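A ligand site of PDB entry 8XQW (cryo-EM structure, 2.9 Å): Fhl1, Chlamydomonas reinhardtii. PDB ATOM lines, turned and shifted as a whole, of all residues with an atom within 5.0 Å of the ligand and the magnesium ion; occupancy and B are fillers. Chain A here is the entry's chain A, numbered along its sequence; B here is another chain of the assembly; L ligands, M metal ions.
An oxygen (O4) of the ligand sits at hydrogen-bond distance from the backbone NH (N) of Lys 505 (2.7 Å). An oxygen (O12) of the ligand sits at hydrogen-bond distance from a ring nitrogen (NE2) of His 643 (2.7 Å). A nitrogen (N4) of the ligand sits close to the backbone carbonyl oxygen (O) of Ala 462 (3.4 Å). An oxygen (O3) of the ligand is in salt-bridge range of the guanidinium group (NH1) of Arg 709 of chain B (3.3 Å). NZ of Lys 505 lies within salt-bridge range of O4 of the ligand (3.1 Å). The backbone NH (N) of Ala 462 sits at hydrogen-bond distance from a nitrogen (N5) of the ligand, at 2.6 Å. The backbone NH (N) of Gly 504 sits at hydrogen-bond distance from an oxygen (O4) of the ligand (2.5 Å). An oxygen (O4) of the ligand is in hydrogen-bond range of the backbone NH (N) of Thr 503. OG1 of Thr 503 lies within hydrogen-bond range of O4 of the ligand (2.9 Å). NH1 of Arg 706 of chain B is in salt-bridge range of O3 of the ligand (3.0 Å). An oxygen (O7) of the ligand is in hydrogen-bond range of the side-chain hydroxyl (OG1) of Thr 506 (2.5 Å). The backbone NH of Thr 506 sits close to an oxygen (O5) of the ligand, 2.9 Å away. The backbone NH (N) of Tyr 507 is in hydrogen-bond range of an oxygen (O7) of the ligand (2.7 Å).
O of Gly 502 sits at hydrogen-bond distance from N of Ala 669, at 3.3 Å. OH of Tyr 507 is in hydrogen-bond range of OH of Tyr 642 (3.2 Å). The guanidinium group of Arg 706 of chain B is in salt-bridge range of the side-chain carboxylate of Asp 679 of chain B, at 2.9 Å. The side-chain hydroxyl (OH) of Tyr 507 is in hydrogen-bond range of the backbone carbonyl oxygen (O) of Asp 460 (2.5 Å). O of Ala 703 of chain B lies within hydrogen-bond range of NH1 of Arg 709 of chain B (3.3 Å). OG1 of Thr 503 sits at hydrogen-bond distance from O of Pro 500. The side-chain amino group (NZ) of Lys 505 is in hydrogen-bond range of the backbone carbonyl oxygen (O) of Pro 500 (2.8 Å). The side-chain hydroxyl (OG1) of Thr 503 lies within hydrogen-bond range of the side-chain amino group (NZ) of Lys 505 (2.7 Å).
N1 of the ligand lies close to N of Gly 502, at 3.2 Å. Ile 461 touches the ligand. Gly 463 touches the ligand (N to N4, 3.8 Å). Met 464 touches the ligand. Pro 501 touches the ligand (CA to O2, 3.6 Å). Ala 669 touches the ligand (CB to C6, 3.8 Å). Ala 670 touches the ligand. Ala 673 touches the ligand (CB to O11, 3.7 Å). Hydrophobic or aromatic side chains that line the ligand: Ala 462, Met 464, Pro 501, Tyr 507, His 643, Ala 669 and Ala 673. Of the 25 residues printed, 17 come within 4 Å of the ligand. The nearest printed residue that does not touch the ligand is Asn 607 (4.1 Å).
Residues that only touch the magnesium ion: Thr 506 (2.7 Å) and Asp 558 (3.8 Å). Of the 25 residues printed, 2 come within 4 Å of the magnesium ion.
The magnesium ion is bound by an oxygen (O1) of the ligand (2.0 Å) and an oxygen (O5) of the ligand (2.5 Å).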
ATOM      1  N   ASP A 460      25.532  -9.366  26.863  1.00  0.00           N
ATOM      2  CA  ASP A 460      24.184  -9.900  26.788  1.00  0.00           C
ATOM      3  C   ASP A 460      23.153  -8.846  26.372  1.00  0.00           C
ATOM      4  O   ASP A 460      21.962  -9.054  26.586  1.00  0.00           O
ATOM      5  CB  ASP A 460      23.788 -10.551  28.119  1.00  0.00           C
ATOM      6  CG  ASP A 460      24.248  -9.768  29.318  1.00  0.00           C
ATOM      7  OD1 ASP A 460      24.231  -8.528  29.247  1.00  0.00           O
ATOM      8  OD2 ASP A 460      24.581 -10.392  30.342  1.00  0.00           O
ATOM      9  N   ILE A 461      23.602  -7.797  25.665  1.00  0.00           N
ATOM     10  CA  ILE A 461      22.674  -6.787  25.071  1.00  0.00           C
ATOM     11  C   ILE A 461      22.987  -6.799  23.569  1.00  0.00           C
ATOM     12  O   ILE A 461      24.071  -6.308  23.197  1.00  0.00           O
ATOM     13  CB  ILE A 461      22.856  -5.383  25.672  1.00  0.00           C
ATOM     14  CG1 ILE A 461      24.302  -5.067  26.000  1.00  0.00           C
ATOM     15  CG2 ILE A 461      21.974  -5.176  26.901  1.00  0.00           C
ATOM     16  CD1 ILE A 461      24.479  -3.686  26.607  1.00  0.00           C
ATOM     17  N   ALA A 462      22.096  -7.344  22.726  1.00  0.00           N
ATOM     18  CA  ALA A 462      22.421  -7.499  21.288  1.00  0.00           C
ATOM     19  C   ALA A 462      21.512  -6.648  20.389  1.00  0.00           C
ATOM     20  O   ALA A 462      20.391  -7.091  20.119  1.00  0.00           O
ATOM     21  CB  ALA A 462      22.271  -8.947  20.926  1.00  0.00           C
ATOM     22  N   GLY A 463      21.976  -5.493  19.936  1.00  0.00           N
ATOM     23  CA  GLY A 463      21.162  -4.699  18.994  1.00  0.00           C
ATOM     24  C   GLY A 463      21.463  -3.218  19.085  1.00  0.00           C
ATOM     25  O   GLY A 463      21.658  -2.596  18.024  1.00  0.00           O
ATOM     26  N   MET A 464      21.524  -2.667  20.298  1.00  0.00           N
ATOM     27  CA  MET A 464      21.724  -1.201  20.457  1.00  0.00           C
ATOM     28  C   MET A 464      23.204  -0.833  20.328  1.00  0.00           C
ATOM     29  O   MET A 464      23.682  -0.067  21.180  1.00  0.00           O
ATOM     30  CB  MET A 464      21.230  -0.745  21.828  1.00  0.00           C
ATOM     31  CG  MET A 464      20.551  -1.840  22.633  1.00  0.00           C
ATOM     32  SD  MET A 464      19.868  -1.176  24.159  1.00  0.00           S
ATOM     33  CE  MET A 464      18.200  -1.832  24.084  1.00  0.00           C
ATOM     34  N   PRO A 500       9.369   3.658  23.004  1.00  0.00           N
ATOM     35  CA  PRO A 500       8.145   2.905  23.261  1.00  0.00           C
ATOM     36  C   PRO A 500       8.391   1.828  24.309  1.00  0.00           C
ATOM     37  O   PRO A 500       9.549   1.527  24.648  1.00  0.00           O
ATOM     38  CB  PRO A 500       7.812   2.295  21.897  1.00  0.00           C
ATOM     39  CG  PRO A 500       8.607   3.077  20.916  1.00  0.00           C
ATOM     40  CD  PRO A 500       9.839   3.488  21.626  1.00  0.00           C
ATOM     41  N   PRO A 501       7.341   1.124  24.821  1.00  0.00           N
ATOM     42  CA  PRO A 501       7.566  -0.007  25.702  1.00  0.00           C
ATOM     43  C   PRO A 501       8.178  -1.214  25.003  1.00  0.00           C
ATOM     44  O   PRO A 501       7.924  -1.387  23.805  1.00  0.00           O
ATOM     45  CB  PRO A 501       6.138  -0.289  26.212  1.00  0.00           C
ATOM     46  CG  PRO A 501       5.254   0.110  25.071  1.00  0.00           C
ATOM     47  CD  PRO A 501       5.891   1.411  24.686  1.00  0.00           C
ATOM     48  N   GLY A 502       8.967  -2.018  25.725  1.00  0.00           N
ATOM     49  CA  GLY A 502       9.558  -3.256  25.180  1.00  0.00           C
ATOM     50  C   GLY A 502      10.837  -3.008  24.431  1.00  0.00           C
ATOM     51  O   GLY A 502      11.301  -3.940  23.763  1.00  0.00           O
ATOM     52  N   THR A 503      11.430  -1.818  24.563  1.00  0.00           N
ATOM     53  CA  THR A 503      12.595  -1.471  23.732  1.00  0.00           C
ATOM     54  C   THR A 503      13.886  -1.947  24.355  1.00  0.00           C
ATOM     55  O   THR A 503      14.727  -2.467  23.605  1.00  0.00           O
ATOM     56  CB  THR A 503      12.598   0.032  23.498  1.00  0.00           C
ATOM     57  OG1 THR A 503      12.075   0.597  24.690  1.00  0.00           O
ATOM     58  CG2 THR A 503      11.750   0.413  22.293  1.00  0.00           C
ATOM     59  N   GLY A 504      14.062  -1.745  25.659  1.00  0.00           N
ATOM     60  CA  GLY A 504      15.259  -2.258  26.334  1.00  0.00           C
ATOM     61  C   GLY A 504      15.932  -1.192  27.150  1.00  0.00           C
ATOM     62  O   GLY A 504      17.163  -1.112  27.120  1.00  0.00           O
ATOM     63  N   LYS A 505      15.160  -0.415  27.886  1.00  0.00           N
ATOM     64  CA  LYS A 505      15.760   0.706  28.653  1.00  0.00           C
ATOM     65  C   LYS A 505      16.183   0.183  30.039  1.00  0.00           C
ATOM     66  O   LYS A 505      17.300   0.508  30.458  1.00  0.00           O
ATOM     67  CB  LYS A 505      14.768   1.860  28.710  1.00  0.00           C
ATOM     68  CG  LYS A 505      14.333   2.416  27.361  1.00  0.00           C
ATOM     69  CD  LYS A 505      13.216   3.448  27.493  1.00  0.00           C
ATOM     70  CE  LYS A 505      11.897   2.829  27.861  1.00  0.00           C
ATOM     71  NZ  LYS A 505      11.265   2.213  26.701  1.00  0.00           N
ATOM     72  N   THR A 506      15.352  -0.620  30.706  1.00  0.00           N
ATOM     73  CA  THR A 506      15.739  -1.217  32.002  1.00  0.00           C
ATOM     74  C   THR A 506      16.827  -2.236  31.785  1.00  0.00           C
ATOM     75  O   THR A 506      17.852  -2.139  32.467  1.00  0.00           O
ATOM     76  CB  THR A 506      14.531  -1.849  32.691  1.00  0.00           C
ATOM     77  OG1 THR A 506      13.737  -2.414  31.658  1.00  0.00           O
ATOM     78  CG2 THR A 506      13.712  -0.815  33.454  1.00  0.00           C
ATOM     79  N   TYR A 507      16.639  -3.183  30.889  1.00  0.00           N
ATOM     80  CA  TYR A 507      17.746  -4.129  30.584  1.00  0.00           C
ATOM     81  C   TYR A 507      19.031  -3.353  30.464  1.00  0.00           C
ATOM     82  O   TYR A 507      20.005  -3.727  31.120  1.00  0.00           O
ATOM     83  CB  TYR A 507      17.535  -4.813  29.240  1.00  0.00           C
ATOM     84  CG  TYR A 507      18.286  -6.114  29.021  1.00  0.00           C
ATOM     85  CD1 TYR A 507      18.531  -6.988  30.065  1.00  0.00           C
ATOM     86  CD2 TYR A 507      18.710  -6.483  27.752  1.00  0.00           C
ATOM     87  CE1 TYR A 507      19.204  -8.180  29.857  1.00  0.00           C
ATOM     88  CE2 TYR A 507      19.376  -7.668  27.530  1.00  0.00           C
ATOM     89  CZ  TYR A 507      19.622  -8.525  28.589  1.00  0.00           C
ATOM     90  OH  TYR A 507      20.284  -9.699  28.375  1.00  0.00           O
ATOM     91  N   ASP A 558      13.736   5.041  37.405  1.00  0.00           N
ATOM     92  CA  ASP A 558      12.897   4.534  36.331  1.00  0.00           C
ATOM     93  C   ASP A 558      11.503   5.152  36.449  1.00  0.00           C
ATOM     94  O   ASP A 558      10.967   5.295  37.548  1.00  0.00           O
ATOM     95  CB  ASP A 558      12.803   3.019  36.399  1.00  0.00           C
ATOM     96  CG  ASP A 558      12.029   2.418  35.244  1.00  0.00           C
ATOM     97  OD1 ASP A 558      11.645   3.168  34.324  1.00  0.00           O
ATOM     98  OD2 ASP A 558      11.785   1.194  35.281  1.00  0.00           O
ATOM     99  N   ASN A 607       8.633   6.304  28.725  1.00  0.00           N
ATOM    100  CA  ASN A 607       7.945   6.109  27.459  1.00  0.00           C
ATOM    101  C   ASN A 607       6.913   7.206  27.228  1.00  0.00           C
ATOM    102  O   ASN A 607       6.145   7.129  26.263  1.00  0.00           O
ATOM    103  CB  ASN A 607       7.278   4.735  27.400  1.00  0.00           C
ATOM    104  CG  ASN A 607       6.661   4.351  28.718  1.00  0.00           C
ATOM    105  OD1 ASN A 607       6.580   5.160  29.636  1.00  0.00           O
ATOM    106  ND2 ASN A 607       6.222   3.107  28.827  1.00  0.00           N
ATOM    107  N   ILE A 639      18.983 -10.117  17.725  1.00  0.00           N
ATOM    108  CA  ILE A 639      18.280 -10.462  18.958  1.00  0.00           C
ATOM    109  C   ILE A 639      17.849 -11.913  18.936  1.00  0.00           C
ATOM    110  O   ILE A 639      18.000 -12.633  19.944  1.00  0.00           O
ATOM    111  CB  ILE A 639      17.081  -9.516  19.169  1.00  0.00           C
ATOM    112  CG1 ILE A 639      17.579  -8.099  19.431  1.00  0.00           C
ATOM    113  CG2 ILE A 639      16.248  -9.986  20.335  1.00  0.00           C
ATOM    114  CD1 ILE A 639      16.475  -7.150  19.786  1.00  0.00           C
ATOM    115  N   TYR A 642      20.954 -14.058  19.659  1.00  0.00           N
ATOM    116  CA  TYR A 642      21.371 -14.117  21.055  1.00  0.00           C
ATOM    117  C   TYR A 642      20.396 -14.942  21.888  1.00  0.00           C
ATOM    118  O   TYR A 642      20.813 -15.759  22.713  1.00  0.00           O
ATOM    119  CB  TYR A 642      21.513 -12.715  21.627  1.00  0.00           C
ATOM    120  CG  TYR A 642      21.470 -12.659  23.130  1.00  0.00           C
ATOM    121  CD1 TYR A 642      22.630 -12.761  23.883  1.00  0.00           C
ATOM    122  CD2 TYR A 642      20.277 -12.486  23.811  1.00  0.00           C
ATOM    123  CE1 TYR A 642      22.593 -12.710  25.251  1.00  0.00           C
ATOM    124  CE2 TYR A 642      20.233 -12.428  25.180  1.00  0.00           C
ATOM    125  CZ  TYR A 642      21.397 -12.541  25.896  1.00  0.00           C
ATOM    126  OH  TYR A 642      21.352 -12.483  27.265  1.00  0.00           O
ATOM    127  N   HIS A 643      19.097 -14.738  21.696  1.00  0.00           N
ATOM    128  CA  HIS A 643      18.100 -15.416  22.508  1.00  0.00           C
ATOM    129  C   HIS A 643      17.812 -16.825  22.038  1.00  0.00           C
ATOM    130  O   HIS A 643      16.806 -17.410  22.444  1.00  0.00           O
ATOM    131  CB  HIS A 643      16.808 -14.610  22.546  1.00  0.00           C
ATOM    132  CG  HIS A 643      16.684 -13.732  23.750  1.00  0.00           C
ATOM    133  ND1 HIS A 643      16.303 -14.222  24.976  1.00  0.00           N
ATOM    134  CD2 HIS A 643      16.911 -12.407  23.923  1.00  0.00           C
ATOM    135  CE1 HIS A 643      16.281 -13.229  25.856  1.00  0.00           C
ATOM    136  NE2 HIS A 643      16.655 -12.117  25.242  1.00  0.00           N
ATOM    137  N   ALA A 669      11.709  -5.935  21.170  1.00  0.00           N
ATOM    138  CA  ALA A 669      12.704  -6.923  21.575  1.00  0.00           C
ATOM    139  C   ALA A 669      12.112  -7.946  22.549  1.00  0.00           C
ATOM    140  O   ALA A 669      12.312  -9.164  22.392  1.00  0.00           O
ATOM    141  CB  ALA A 669      13.910  -6.228  22.200  1.00  0.00           C
ATOM    142  N   ALA A 670      11.395  -7.455  23.555  1.00  0.00           N
ATOM    143  CA  ALA A 670      10.728  -8.349  24.499  1.00  0.00           C
ATOM    144  C   ALA A 670       9.830  -9.328  23.767  1.00  0.00           C
ATOM    145  O   ALA A 670       9.739 -10.502  24.165  1.00  0.00           O
ATOM    146  CB  ALA A 670       9.919  -7.543  25.505  1.00  0.00           C
ATOM    147  N   ALA A 673      11.984 -12.155  22.286  1.00  0.00           N
ATOM    148  CA  ALA A 673      12.399 -13.059  23.347  1.00  0.00           C
ATOM    149  C   ALA A 673      11.257 -13.983  23.753  1.00  0.00           C
ATOM    150  O   ALA A 673      11.429 -15.207  23.871  1.00  0.00           O
ATOM    151  CB  ALA A 673      12.903 -12.268  24.555  1.00  0.00           C
ATOM    152  N   ASP B 679       7.816  -6.312  35.829  1.00  0.00           N
ATOM    153  CA  ASP B 679       9.197  -6.372  35.364  1.00  0.00           C
ATOM    154  C   ASP B 679      10.108  -5.456  36.185  1.00  0.00           C
ATOM    155  O   ASP B 679      11.008  -5.936  36.876  1.00  0.00           O
ATOM    156  CB  ASP B 679       9.270  -6.014  33.883  1.00  0.00           C
ATOM    157  CG  ASP B 679       9.460  -7.227  33.003  1.00  0.00           C
ATOM    158  OD1 ASP B 679       9.791  -8.300  33.544  1.00  0.00           O
ATOM    159  OD2 ASP B 679       9.268  -7.118  31.779  1.00  0.00           O
ATOM    160  N   ALA B 703       1.757  -0.547  27.841  1.00  0.00           N
ATOM    161  CA  ALA B 703       2.853  -1.182  28.564  1.00  0.00           C
ATOM    162  C   ALA B 703       2.393  -2.434  29.296  1.00  0.00           C
ATOM    163  O   ALA B 703       3.170  -3.381  29.464  1.00  0.00           O
ATOM    164  CB  ALA B 703       3.480  -0.190  29.538  1.00  0.00           C
ATOM    165  N   ARG B 706       2.129  -5.854  27.165  1.00  0.00           N
ATOM    166  CA  ARG B 706       3.314  -6.174  26.320  1.00  0.00           C
ATOM    167  C   ARG B 706       3.901  -7.544  26.632  1.00  0.00           C
ATOM    168  O   ARG B 706       3.972  -7.909  27.819  1.00  0.00           O
ATOM    169  CB  ARG B 706       4.398  -5.098  26.502  1.00  0.00           C
ATOM    170  CG  ARG B 706       5.168  -5.103  27.816  1.00  0.00           C
ATOM    171  CD  ARG B 706       6.394  -4.226  27.729  1.00  0.00           C
ATOM    172  NE  ARG B 706       7.618  -5.038  27.788  1.00  0.00           N
ATOM    173  CZ  ARG B 706       8.250  -5.319  28.915  1.00  0.00           C
ATOM    174  NH1 ARG B 706       8.014  -4.606  30.001  1.00  0.00           N
ATOM    175  NH2 ARG B 706       9.117  -6.312  28.956  1.00  0.00           N
ATOM    176  N   ARG B 709       5.434  -8.816  30.315  1.00  0.00           N
ATOM    177  CA  ARG B 709       4.690  -8.566  31.542  1.00  0.00           C
ATOM    178  C   ARG B 709       3.466  -9.457  31.664  1.00  0.00           C
ATOM    179  O   ARG B 709       3.058  -9.789  32.785  1.00  0.00           O
ATOM    180  CB  ARG B 709       4.265  -7.103  31.636  1.00  0.00           C
ATOM    181  CG  ARG B 709       5.345  -6.196  32.163  1.00  0.00           C
ATOM    182  CD  ARG B 709       4.964  -4.737  32.087  1.00  0.00           C
ATOM    183  NE  ARG B 709       5.996  -3.907  32.694  1.00  0.00           N
ATOM    184  CZ  ARG B 709       6.244  -2.654  32.340  1.00  0.00           C
ATOM    185  NH1 ARG B 709       5.545  -2.081  31.375  1.00  0.00           N
ATOM    186  NH2 ARG B 709       7.204  -1.974  32.944  1.00  0.00           N
HETATM  187  P1  LIG L   1       9.422  -1.011  29.351  1.00  0.00           P
HETATM  188  O1  LIG L   1       9.838  -0.962  30.794  1.00  0.00           O
HETATM  189  O2  LIG L   1       9.257   0.389  28.881  1.00  0.00           O
HETATM  190  O3  LIG L   1       8.096  -1.691  29.255  1.00  0.00           O
HETATM  191  P2  LIG L   1      12.122  -1.456  28.438  1.00  0.00           P
HETATM  192  O4  LIG L   1      12.494  -0.587  27.281  1.00  0.00           O
HETATM  193  O5  LIG L   1      12.637  -1.097  29.801  1.00  0.00           O
HETATM  194  N1  LIG L   1      10.535  -1.811  28.473  1.00  0.00           N
HETATM  195  P3  LIG L   1      13.015  -4.159  28.972  1.00  0.00           P
HETATM  196  O6  LIG L   1      11.749  -4.470  29.689  1.00  0.00           O
HETATM  197  O7  LIG L   1      14.262  -3.969  29.770  1.00  0.00           O
HETATM  198  O8  LIG L   1      12.791  -2.854  28.077  1.00  0.00           O
HETATM  199  O9  LIG L   1      13.283  -5.273  27.858  1.00  0.00           O
HETATM  200  C1  LIG L   1      14.087  -6.398  28.280  1.00  0.00           C
HETATM  201  C2  LIG L   1      13.706  -7.614  27.478  1.00  0.00           C
HETATM  202  O10 LIG L   1      14.042  -7.380  26.103  1.00  0.00           O
HETATM  203  C3  LIG L   1      14.450  -8.905  27.833  1.00  0.00           C
HETATM  204  O11 LIG L   1      13.770 -10.034  27.333  1.00  0.00           O
HETATM  205  C4  LIG L   1      15.760  -8.682  27.070  1.00  0.00           C
HETATM  206  O12 LIG L   1      16.466  -9.880  26.820  1.00  0.00           O
HETATM  207  C5  LIG L   1      15.230  -8.070  25.778  1.00  0.00           C
HETATM  208  N2  LIG L   1      16.140  -7.125  25.183  1.00  0.00           N
HETATM  209  C6  LIG L   1      16.078  -5.754  25.225  1.00  0.00           C
HETATM  210  N3  LIG L   1      17.075  -5.190  24.584  1.00  0.00           N
HETATM  211  C7  LIG L   1      17.836  -6.253  24.116  1.00  0.00           C
HETATM  212  C8  LIG L   1      19.019  -6.311  23.363  1.00  0.00           C
HETATM  213  N4  LIG L   1      19.677  -5.235  22.932  1.00  0.00           N
HETATM  214  N5  LIG L   1      19.502  -7.542  23.063  1.00  0.00           N
HETATM  215  C9  LIG L   1      18.836  -8.612  23.494  1.00  0.00           C
HETATM  216  N6  LIG L   1      17.719  -8.678  24.200  1.00  0.00           N
HETATM  217  C10 LIG L   1      17.265  -7.442  24.479  1.00  0.00           C
HETATM  218 MG    MG M   1      11.460  -0.623  31.971  1.00  0.00          MG
